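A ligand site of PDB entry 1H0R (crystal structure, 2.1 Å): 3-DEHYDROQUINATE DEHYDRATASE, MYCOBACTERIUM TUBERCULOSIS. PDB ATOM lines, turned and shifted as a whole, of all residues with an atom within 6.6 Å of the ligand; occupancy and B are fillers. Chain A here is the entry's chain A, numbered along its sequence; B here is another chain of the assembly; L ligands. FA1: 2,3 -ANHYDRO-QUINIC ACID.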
ATOM      1  N   PRO A  11     -30.530 -22.454 -24.790  1.00  0.00           N
ATOM      2  CA  PRO A  11     -31.332 -21.836 -25.845  1.00  0.00           C
ATOM      3  C   PRO A  11     -31.248 -22.507 -27.198  1.00  0.00           C
ATOM      4  O   PRO A  11     -30.153 -22.925 -27.636  1.00  0.00           O
ATOM      5  CB  PRO A  11     -30.782 -20.394 -25.929  1.00  0.00           C
ATOM      6  CG  PRO A  11     -29.803 -20.296 -24.856  1.00  0.00           C
ATOM      7  CD  PRO A  11     -29.591 -21.498 -24.153  1.00  0.00           C
ATOM      8  N   ASN A  12     -32.398 -22.566 -27.869  1.00  0.00           N
ATOM      9  CA  ASN A  12     -32.542 -23.159 -29.198  1.00  0.00           C
ATOM     10  C   ASN A  12     -32.614 -24.706 -29.290  1.00  0.00           C
ATOM     11  O   ASN A  12     -32.937 -25.260 -30.349  1.00  0.00           O
ATOM     12  CB  ASN A  12     -31.519 -22.624 -30.244  1.00  0.00           C
ATOM     13  CG  ASN A  12     -31.544 -21.103 -30.402  1.00  0.00           C
ATOM     14  OD1 ASN A  12     -32.588 -20.523 -30.421  1.00  0.00           O
ATOM     15  ND2 ASN A  12     -30.406 -20.479 -30.494  1.00  0.00           N
ATOM     16  N   LEU A  13     -32.318 -25.386 -28.208  1.00  0.00           N
ATOM     17  CA  LEU A  13     -32.327 -26.840 -28.198  1.00  0.00           C
ATOM     18  C   LEU A  13     -33.736 -27.382 -28.171  1.00  0.00           C
ATOM     19  O   LEU A  13     -33.961 -28.530 -28.547  1.00  0.00           O
ATOM     20  CB  LEU A  13     -31.450 -27.294 -27.055  1.00  0.00           C
ATOM     21  CG  LEU A  13     -30.011 -27.040 -27.538  1.00  0.00           C
ATOM     22  CD1 LEU A  13     -29.018 -26.818 -26.385  1.00  0.00           C
ATOM     23  CD2 LEU A  13     -29.596 -28.227 -28.448  1.00  0.00           C
ATOM     24  N   VAL A  23     -26.748 -29.932 -38.832  1.00  0.00           N
ATOM     25  CA  VAL A  23     -25.731 -29.666 -37.793  1.00  0.00           C
ATOM     26  C   VAL A  23     -26.008 -30.468 -36.486  1.00  0.00           C
ATOM     27  O   VAL A  23     -25.127 -31.160 -35.950  1.00  0.00           O
ATOM     28  CB  VAL A  23     -25.696 -28.148 -37.447  1.00  0.00           C
ATOM     29  CG1 VAL A  23     -24.625 -27.823 -36.376  1.00  0.00           C
ATOM     30  CG2 VAL A  23     -25.536 -27.309 -38.760  1.00  0.00           C
ATOM     31  N   TYR A  24     -27.255 -30.341 -36.008  1.00  0.00           N
ATOM     32  CA  TYR A  24     -27.752 -31.001 -34.795  1.00  0.00           C
ATOM     33  C   TYR A  24     -28.612 -32.286 -35.058  1.00  0.00           C
ATOM     34  O   TYR A  24     -29.020 -32.974 -34.077  1.00  0.00           O
ATOM     35  CB  TYR A  24     -28.468 -29.977 -33.880  1.00  0.00           C
ATOM     36  CG  TYR A  24     -27.726 -28.651 -33.764  1.00  0.00           C
ATOM     37  CD1 TYR A  24     -28.107 -27.554 -34.562  1.00  0.00           C
ATOM     38  CD2 TYR A  24     -26.612 -28.498 -32.904  1.00  0.00           C
ATOM     39  CE1 TYR A  24     -27.419 -26.340 -34.514  1.00  0.00           C
ATOM     40  CE2 TYR A  24     -25.881 -27.251 -32.864  1.00  0.00           C
ATOM     41  CZ  TYR A  24     -26.288 -26.173 -33.653  1.00  0.00           C
ATOM     42  OH  TYR A  24     -25.682 -24.910 -33.682  1.00  0.00           O
ATOM     43  N   ASN A  75     -25.875 -28.966 -21.832  1.00  0.00           N
ATOM     44  CA  ASN A  75     -25.631 -28.459 -23.200  1.00  0.00           C
ATOM     45  C   ASN A  75     -26.162 -27.066 -23.208  1.00  0.00           C
ATOM     46  O   ASN A  75     -27.392 -26.895 -23.336  1.00  0.00           O
ATOM     47  CB  ASN A  75     -26.340 -29.276 -24.280  1.00  0.00           C
ATOM     48  CG  ASN A  75     -26.004 -28.792 -25.634  1.00  0.00           C
ATOM     49  OD1 ASN A  75     -25.495 -27.626 -25.814  1.00  0.00           O
ATOM     50  ND2 ASN A  75     -26.225 -29.660 -26.619  1.00  0.00           N
ATOM     51  N   ALA A  76     -25.290 -26.084 -22.983  1.00  0.00           N
ATOM     52  CA  ALA A  76     -25.732 -24.690 -22.827  1.00  0.00           C
ATOM     53  C   ALA A  76     -26.022 -23.923 -24.131  1.00  0.00           C
ATOM     54  O   ALA A  76     -26.364 -22.719 -24.131  1.00  0.00           O
ATOM     55  CB  ALA A  76     -24.716 -23.951 -22.052  1.00  0.00           C
ATOM     56  N   GLY A  77     -25.811 -24.589 -25.259  1.00  0.00           N
ATOM     57  CA  GLY A  77     -25.978 -23.945 -26.564  1.00  0.00           C
ATOM     58  C   GLY A  77     -25.015 -22.776 -26.743  1.00  0.00           C
ATOM     59  O   GLY A  77     -23.841 -22.826 -26.353  1.00  0.00           O
ATOM     60  N   GLY A  78     -25.515 -21.655 -27.239  1.00  0.00           N
ATOM     61  CA  GLY A  78     -24.673 -20.519 -27.443  1.00  0.00           C
ATOM     62  C   GLY A  78     -24.047 -19.880 -26.215  1.00  0.00           C
ATOM     63  O   GLY A  78     -22.994 -19.264 -26.338  1.00  0.00           O
ATOM     64  N   LEU A  79     -24.724 -19.989 -25.071  1.00  0.00           N
ATOM     65  CA  LEU A  79     -24.292 -19.505 -23.808  1.00  0.00           C
ATOM     66  C   LEU A  79     -22.965 -20.084 -23.370  1.00  0.00           C
ATOM     67  O   LEU A  79     -22.251 -19.497 -22.537  1.00  0.00           O
ATOM     68  CB  LEU A  79     -25.410 -19.779 -22.799  1.00  0.00           C
ATOM     69  CG  LEU A  79     -26.716 -19.046 -22.958  1.00  0.00           C
ATOM     70  CD1 LEU A  79     -27.635 -19.299 -21.793  1.00  0.00           C
ATOM     71  CD2 LEU A  79     -26.551 -17.620 -23.147  1.00  0.00           C
ATOM     72  N   THR A  80     -22.634 -21.272 -23.906  1.00  0.00           N
ATOM     73  CA  THR A  80     -21.303 -21.888 -23.730  1.00  0.00           C
ATOM     74  C   THR A  80     -20.118 -20.914 -23.897  1.00  0.00           C
ATOM     75  O   THR A  80     -19.127 -20.909 -23.116  1.00  0.00           O
ATOM     76  CB  THR A  80     -21.169 -23.006 -24.740  1.00  0.00           C
ATOM     77  OG1 THR A  80     -22.171 -23.978 -24.486  1.00  0.00           O
ATOM     78  CG2 THR A  80     -19.852 -23.742 -24.622  1.00  0.00           C
ATOM     79  N   HIS A  81     -20.232 -20.108 -24.912  1.00  0.00           N
ATOM     80  CA  HIS A  81     -19.173 -19.253 -25.405  1.00  0.00           C
ATOM     81  C   HIS A  81     -19.275 -17.807 -24.875  1.00  0.00           C
ATOM     82  O   HIS A  81     -18.340 -17.052 -25.120  1.00  0.00           O
ATOM     83  CB  HIS A  81     -19.220 -19.179 -26.926  1.00  0.00           C
ATOM     84  CG  HIS A  81     -19.444 -20.487 -27.558  1.00  0.00           C
ATOM     85  ND1 HIS A  81     -18.619 -21.554 -27.348  1.00  0.00           N
ATOM     86  CD2 HIS A  81     -20.412 -20.925 -28.421  1.00  0.00           C
ATOM     87  CE1 HIS A  81     -19.050 -22.597 -28.053  1.00  0.00           C
ATOM     88  NE2 HIS A  81     -20.145 -22.251 -28.690  1.00  0.00           N
ATOM     89  N   VAL A 100     -21.875 -31.169 -22.604  1.00  0.00           N
ATOM     90  CA  VAL A 100     -22.160 -31.850 -23.836  1.00  0.00           C
ATOM     91  C   VAL A 100     -22.418 -30.879 -24.971  1.00  0.00           C
ATOM     92  O   VAL A 100     -23.190 -29.950 -24.843  1.00  0.00           O
ATOM     93  CB  VAL A 100     -23.363 -32.818 -23.738  1.00  0.00           C
ATOM     94  CG1 VAL A 100     -23.778 -33.362 -25.177  1.00  0.00           C
ATOM     95  CG2 VAL A 100     -23.000 -34.029 -22.922  1.00  0.00           C
ATOM     96  N   HIS A 101     -21.867 -31.202 -26.131  1.00  0.00           N
ATOM     97  CA  HIS A 101     -22.238 -30.551 -27.418  1.00  0.00           C
ATOM     98  C   HIS A 101     -22.556 -31.597 -28.506  1.00  0.00           C
ATOM     99  O   HIS A 101     -21.767 -32.503 -28.754  1.00  0.00           O
ATOM    100  CB  HIS A 101     -21.148 -29.631 -27.857  1.00  0.00           C
ATOM    101  CG  HIS A 101     -20.799 -28.573 -26.855  1.00  0.00           C
ATOM    102  ND1 HIS A 101     -21.531 -27.419 -26.703  1.00  0.00           N
ATOM    103  CD2 HIS A 101     -19.800 -28.510 -25.945  1.00  0.00           C
ATOM    104  CE1 HIS A 101     -20.992 -26.698 -25.732  1.00  0.00           C
ATOM    105  NE2 HIS A 101     -19.955 -27.344 -25.244  1.00  0.00           N
ATOM    106  N   ILE A 102     -23.665 -31.442 -29.207  1.00  0.00           N
ATOM    107  CA  ILE A 102     -24.087 -32.426 -30.201  1.00  0.00           C
ATOM    108  C   ILE A 102     -23.149 -32.347 -31.433  1.00  0.00           C
ATOM    109  O   ILE A 102     -22.690 -33.386 -31.982  1.00  0.00           O
ATOM    110  CB  ILE A 102     -25.596 -32.100 -30.605  1.00  0.00           C
ATOM    111  CG1 ILE A 102     -26.540 -32.421 -29.444  1.00  0.00           C
ATOM    112  CG2 ILE A 102     -26.136 -32.841 -31.882  1.00  0.00           C
ATOM    113  CD1 ILE A 102     -27.874 -31.818 -29.581  1.00  0.00           C
ATOM    114  N   SER A 103     -22.893 -31.117 -31.932  1.00  0.00           N
ATOM    115  CA  SER A 103     -21.994 -30.935 -33.050  1.00  0.00           C
ATOM    116  C   SER A 103     -20.528 -30.864 -32.616  1.00  0.00           C
ATOM    117  O   SER A 103     -20.176 -30.651 -31.420  1.00  0.00           O
ATOM    118  CB  SER A 103     -22.375 -29.649 -33.825  1.00  0.00           C
ATOM    119  OG  SER A 103     -21.924 -28.473 -33.147  1.00  0.00           O
ATOM    120  N   ASN A 104     -19.613 -31.046 -33.569  1.00  0.00           N
ATOM    121  CA  ASN A 104     -18.235 -30.795 -33.260  1.00  0.00           C
ATOM    122  C   ASN A 104     -17.917 -29.292 -33.304  1.00  0.00           C
ATOM    123  O   ASN A 104     -17.650 -28.791 -34.379  1.00  0.00           O
ATOM    124  CB  ASN A 104     -17.331 -31.549 -34.227  1.00  0.00           C
ATOM    125  CG  ASN A 104     -15.876 -31.483 -33.841  1.00  0.00           C
ATOM    126  OD1 ASN A 104     -15.433 -30.649 -33.005  1.00  0.00           O
ATOM    127  ND2 ASN A 104     -15.082 -32.347 -34.466  1.00  0.00           N
ATOM    128  N   VAL A 105     -17.911 -28.615 -32.185  1.00  0.00           N
ATOM    129  CA  VAL A 105     -17.665 -27.161 -32.097  1.00  0.00           C
ATOM    130  C   VAL A 105     -16.270 -26.751 -32.608  1.00  0.00           C
ATOM    131  O   VAL A 105     -15.997 -25.581 -32.759  1.00  0.00           O
ATOM    132  CB  VAL A 105     -17.822 -26.669 -30.638  1.00  0.00           C
ATOM    133  CG1 VAL A 105     -19.287 -26.827 -30.149  1.00  0.00           C
ATOM    134  CG2 VAL A 105     -16.903 -27.435 -29.715  1.00  0.00           C
ATOM    135  N   ARG A 108     -16.096 -25.806 -36.736  1.00  0.00           N
ATOM    136  CA  ARG A 108     -16.992 -24.730 -37.131  1.00  0.00           C
ATOM    137  C   ARG A 108     -16.254 -23.397 -37.044  1.00  0.00           C
ATOM    138  O   ARG A 108     -15.084 -23.364 -37.344  1.00  0.00           O
ATOM    139  CB  ARG A 108     -18.302 -24.782 -36.250  1.00  0.00           C
ATOM    140  CG  ARG A 108     -19.037 -26.132 -36.457  1.00  0.00           C
ATOM    141  CD  ARG A 108     -20.305 -26.343 -35.630  1.00  0.00           C
ATOM    142  NE  ARG A 108     -21.290 -25.318 -35.993  1.00  0.00           N
ATOM    143  CZ  ARG A 108     -22.386 -25.002 -35.289  1.00  0.00           C
ATOM    144  NH1 ARG A 108     -22.717 -25.600 -34.128  1.00  0.00           N
ATOM    145  NH2 ARG A 108     -23.131 -24.029 -35.740  1.00  0.00           N
ATOM    146  N   PHE A 111     -14.845 -18.937 -33.071  1.00  0.00           N
ATOM    147  CA  PHE A 111     -15.399 -18.471 -31.788  1.00  0.00           C
ATOM    148  C   PHE A 111     -16.110 -19.617 -31.001  1.00  0.00           C
ATOM    149  O   PHE A 111     -16.216 -19.523 -29.815  1.00  0.00           O
ATOM    150  CB  PHE A 111     -16.321 -17.225 -31.941  1.00  0.00           C
ATOM    151  CG  PHE A 111     -17.655 -17.517 -32.645  1.00  0.00           C
ATOM    152  CD1 PHE A 111     -18.675 -18.224 -32.013  1.00  0.00           C
ATOM    153  CD2 PHE A 111     -17.839 -17.092 -33.944  1.00  0.00           C
ATOM    154  CE1 PHE A 111     -19.851 -18.503 -32.705  1.00  0.00           C
ATOM    155  CE2 PHE A 111     -19.029 -17.335 -34.610  1.00  0.00           C
ATOM    156  CZ  PHE A 111     -20.028 -17.995 -34.024  1.00  0.00           C
ATOM    157  N   ARG A 112     -16.409 -20.748 -31.636  1.00  0.00           N
ATOM    158  CA  ARG A 112     -17.039 -21.874 -30.929  1.00  0.00           C
ATOM    159  C   ARG A 112     -16.037 -22.787 -30.269  1.00  0.00           C
ATOM    160  O   ARG A 112     -16.408 -23.718 -29.517  1.00  0.00           O
ATOM    161  CB  ARG A 112     -17.881 -22.689 -31.844  1.00  0.00           C
ATOM    162  CG  ARG A 112     -19.159 -21.985 -32.281  1.00  0.00           C
ATOM    163  CD  ARG A 112     -20.058 -22.896 -33.248  1.00  0.00           C
ATOM    164  NE  ARG A 112     -20.938 -22.101 -34.051  1.00  0.00           N
ATOM    165  CZ  ARG A 112     -22.055 -21.562 -33.639  1.00  0.00           C
ATOM    166  NH1 ARG A 112     -22.584 -21.823 -32.414  1.00  0.00           N
ATOM    167  NH2 ARG A 112     -22.729 -20.831 -34.503  1.00  0.00           N
ATOM    168  N   GLY A 127     -19.335 -33.511 -30.576  1.00  0.00           N
ATOM    169  CA  GLY A 127     -19.394 -34.161 -31.857  1.00  0.00           C
ATOM    170  C   GLY A 127     -19.907 -35.557 -31.952  1.00  0.00           C
ATOM    171  O   GLY A 127     -19.847 -36.104 -33.054  1.00  0.00           O
ATOM    172  N   TYR A 133     -25.100 -37.462 -24.852  1.00  0.00           N
ATOM    173  CA  TYR A 133     -25.889 -37.447 -23.622  1.00  0.00           C
ATOM    174  C   TYR A 133     -25.930 -38.811 -22.953  1.00  0.00           C
ATOM    175  O   TYR A 133     -25.858 -38.886 -21.748  1.00  0.00           O
ATOM    176  CB  TYR A 133     -27.309 -36.972 -23.867  1.00  0.00           C
ATOM    177  CG  TYR A 133     -27.546 -35.564 -24.367  1.00  0.00           C
ATOM    178  CD1 TYR A 133     -27.773 -34.550 -23.479  1.00  0.00           C
ATOM    179  CD2 TYR A 133     -27.614 -35.254 -25.754  1.00  0.00           C
ATOM    180  CE1 TYR A 133     -27.986 -33.283 -23.884  1.00  0.00           C
ATOM    181  CE2 TYR A 133     -27.846 -33.965 -26.154  1.00  0.00           C
ATOM    182  CZ  TYR A 133     -28.049 -32.985 -25.205  1.00  0.00           C
ATOM    183  OH  TYR A 133     -28.288 -31.688 -25.483  1.00  0.00           O
ATOM    184  N   VAL B  84     -24.342 -15.278 -29.106  1.00  0.00           N
ATOM    185  CA  VAL B  84     -24.253 -16.401 -30.085  1.00  0.00           C
ATOM    186  C   VAL B  84     -25.582 -17.115 -30.184  1.00  0.00           C
ATOM    187  O   VAL B  84     -26.005 -17.533 -31.273  1.00  0.00           O
ATOM    188  CB  VAL B  84     -23.131 -17.388 -29.741  1.00  0.00           C
ATOM    189  CG1 VAL B  84     -23.222 -18.628 -30.638  1.00  0.00           C
ATOM    190  CG2 VAL B  84     -21.852 -16.617 -29.768  1.00  0.00           C
ATOM    191  N   ALA B  85     -26.311 -17.172 -29.085  1.00  0.00           N
ATOM    192  CA  ALA B  85     -27.667 -17.729 -29.158  1.00  0.00           C
ATOM    193  C   ALA B  85     -28.619 -17.044 -30.164  1.00  0.00           C
ATOM    194  O   ALA B  85     -29.303 -17.723 -30.921  1.00  0.00           O
ATOM    195  CB  ALA B  85     -28.280 -17.799 -27.784  1.00  0.00           C
ATOM    196  N   ASP B  88     -27.529 -17.978 -33.680  1.00  0.00           N
ATOM    197  CA  ASP B  88     -27.892 -19.321 -34.121  1.00  0.00           C
ATOM    198  C   ASP B  88     -29.383 -19.387 -34.487  1.00  0.00           C
ATOM    199  O   ASP B  88     -29.772 -20.068 -35.436  1.00  0.00           O
ATOM    200  CB  ASP B  88     -27.586 -20.361 -33.030  1.00  0.00           C
ATOM    201  CG  ASP B  88     -26.075 -20.581 -32.870  1.00  0.00           C
ATOM    202  OD1 ASP B  88     -25.269 -20.196 -33.753  1.00  0.00           O
ATOM    203  OD2 ASP B  88     -25.655 -21.165 -31.894  1.00  0.00           O
HETATM  204  C2  FA1 L   1     -22.834 -25.985 -30.092  1.00  0.00           C
HETATM  205  C3  FA1 L   1     -22.888 -24.493 -29.759  1.00  0.00           C
HETATM  206  O3  FA1 L   1     -21.778 -23.830 -30.428  1.00  0.00           O
HETATM  207  C4  FA1 L   1     -24.203 -23.916 -30.344  1.00  0.00           C
HETATM  208  O4  FA1 L   1     -24.260 -22.531 -30.036  1.00  0.00           O
HETATM  209  C5  FA1 L   1     -25.470 -24.714 -30.042  1.00  0.00           C
HETATM  210  C6  FA1 L   1     -25.392 -25.971 -29.755  1.00  0.00           C
HETATM  211  C   FA1 L   1     -24.228 -28.118 -29.939  1.00  0.00           C
HETATM  212  O1  FA1 L   1     -23.519 -28.593 -30.885  1.00  0.00           O
HETATM  213  O30 FA1 L   1     -23.787 -26.624 -28.086  1.00  0.00           O
HETATM  214  O2  FA1 L   1     -25.018 -28.912 -29.256  1.00  0.00           O
HETATM  215  C1  FA1 L   1     -24.073 -26.682 -29.519  1.00  0.00           C
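OD2 of Asp 88 of chain B sits at hydrogen-bond distance from O4 of the ligand (2.7 Å).
The backbone NH (N) of Ser 103 is in hydrogen-bond range of an oxygen (O1) of the ligand (2.8 Å).
ND2 of Asn 75 sits at hydrogen-bond distance from O2 of the ligand (3.0 Å).
An oxygen (O3) of the ligand sits at hydrogen-bond distance from the guanidinium group (NH1) of Arg 112, 2.9 Å away.
O4 of the ligand is in hydrogen-bond range of N of Gly 78 (3.2 Å).
O2 of the ligand sits at hydrogen-bond distance from N of Ile 102 (2.9 Å).
NE2 of His 81 lies within hydrogen-bond range of O3 of the ligand, 2.9 Å away.
The side-chain hydroxyl (OG) of Ser 103 sits at hydrogen-bond distance from an oxygen (O1) of the ligand (2.8 Å).
An oxygen (O30) of the ligand is in hydrogen-bond range of a ring nitrogen (ND1) of His 101.
O of Gly 77 is in hydrogen-bond range of OG1 of Thr 80 (2.8 Å).
The side-chain hydroxyl of Tyr 24 sits at hydrogen-bond distance from the guanidinium group of Arg 108, 3.1 Å away.
N of Gly 127 sits at hydrogen-bond distance from O of Ser 103, 3.1 Å away.
OD1 of Asn 75 lies close to O of Val 100, at 3.4 Å.
The side-chain amide nitrogen (ND2) of Asn 75 is in hydrogen-bond range of the side-chain hydroxyl (OH) of Tyr 133 (3.1 Å).
The side-chain amide oxygen of Asn 75 sits at hydrogen-bond distance from the backbone NH of Gly 77, at 3.1 Å.
OD1 of Asp 88 of chain B lies within salt-bridge range of NH2 of Arg 112.
N of Gly 127 is in hydrogen-bond range of O of His 101, 3.2 Å away.
Residues that only touch the ligand: Tyr 24, Gly 77 and Val 105.
Hydrophobic or aromatic side chains within 4 Å of the ligand: Tyr 24, His 81, His 101, Ile 102 and Val 105.
11 residues have an atom within 4 Å of the ligand: Tyr 24, Asn 75, Gly 77, Gly 78, His 81, His 101, Ile 102, Ser 103, Val 105, Arg 112 and Asp 88 of chain B.
The nearest printed residue that does not touch the ligand is Arg 108 (4.1 Å).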
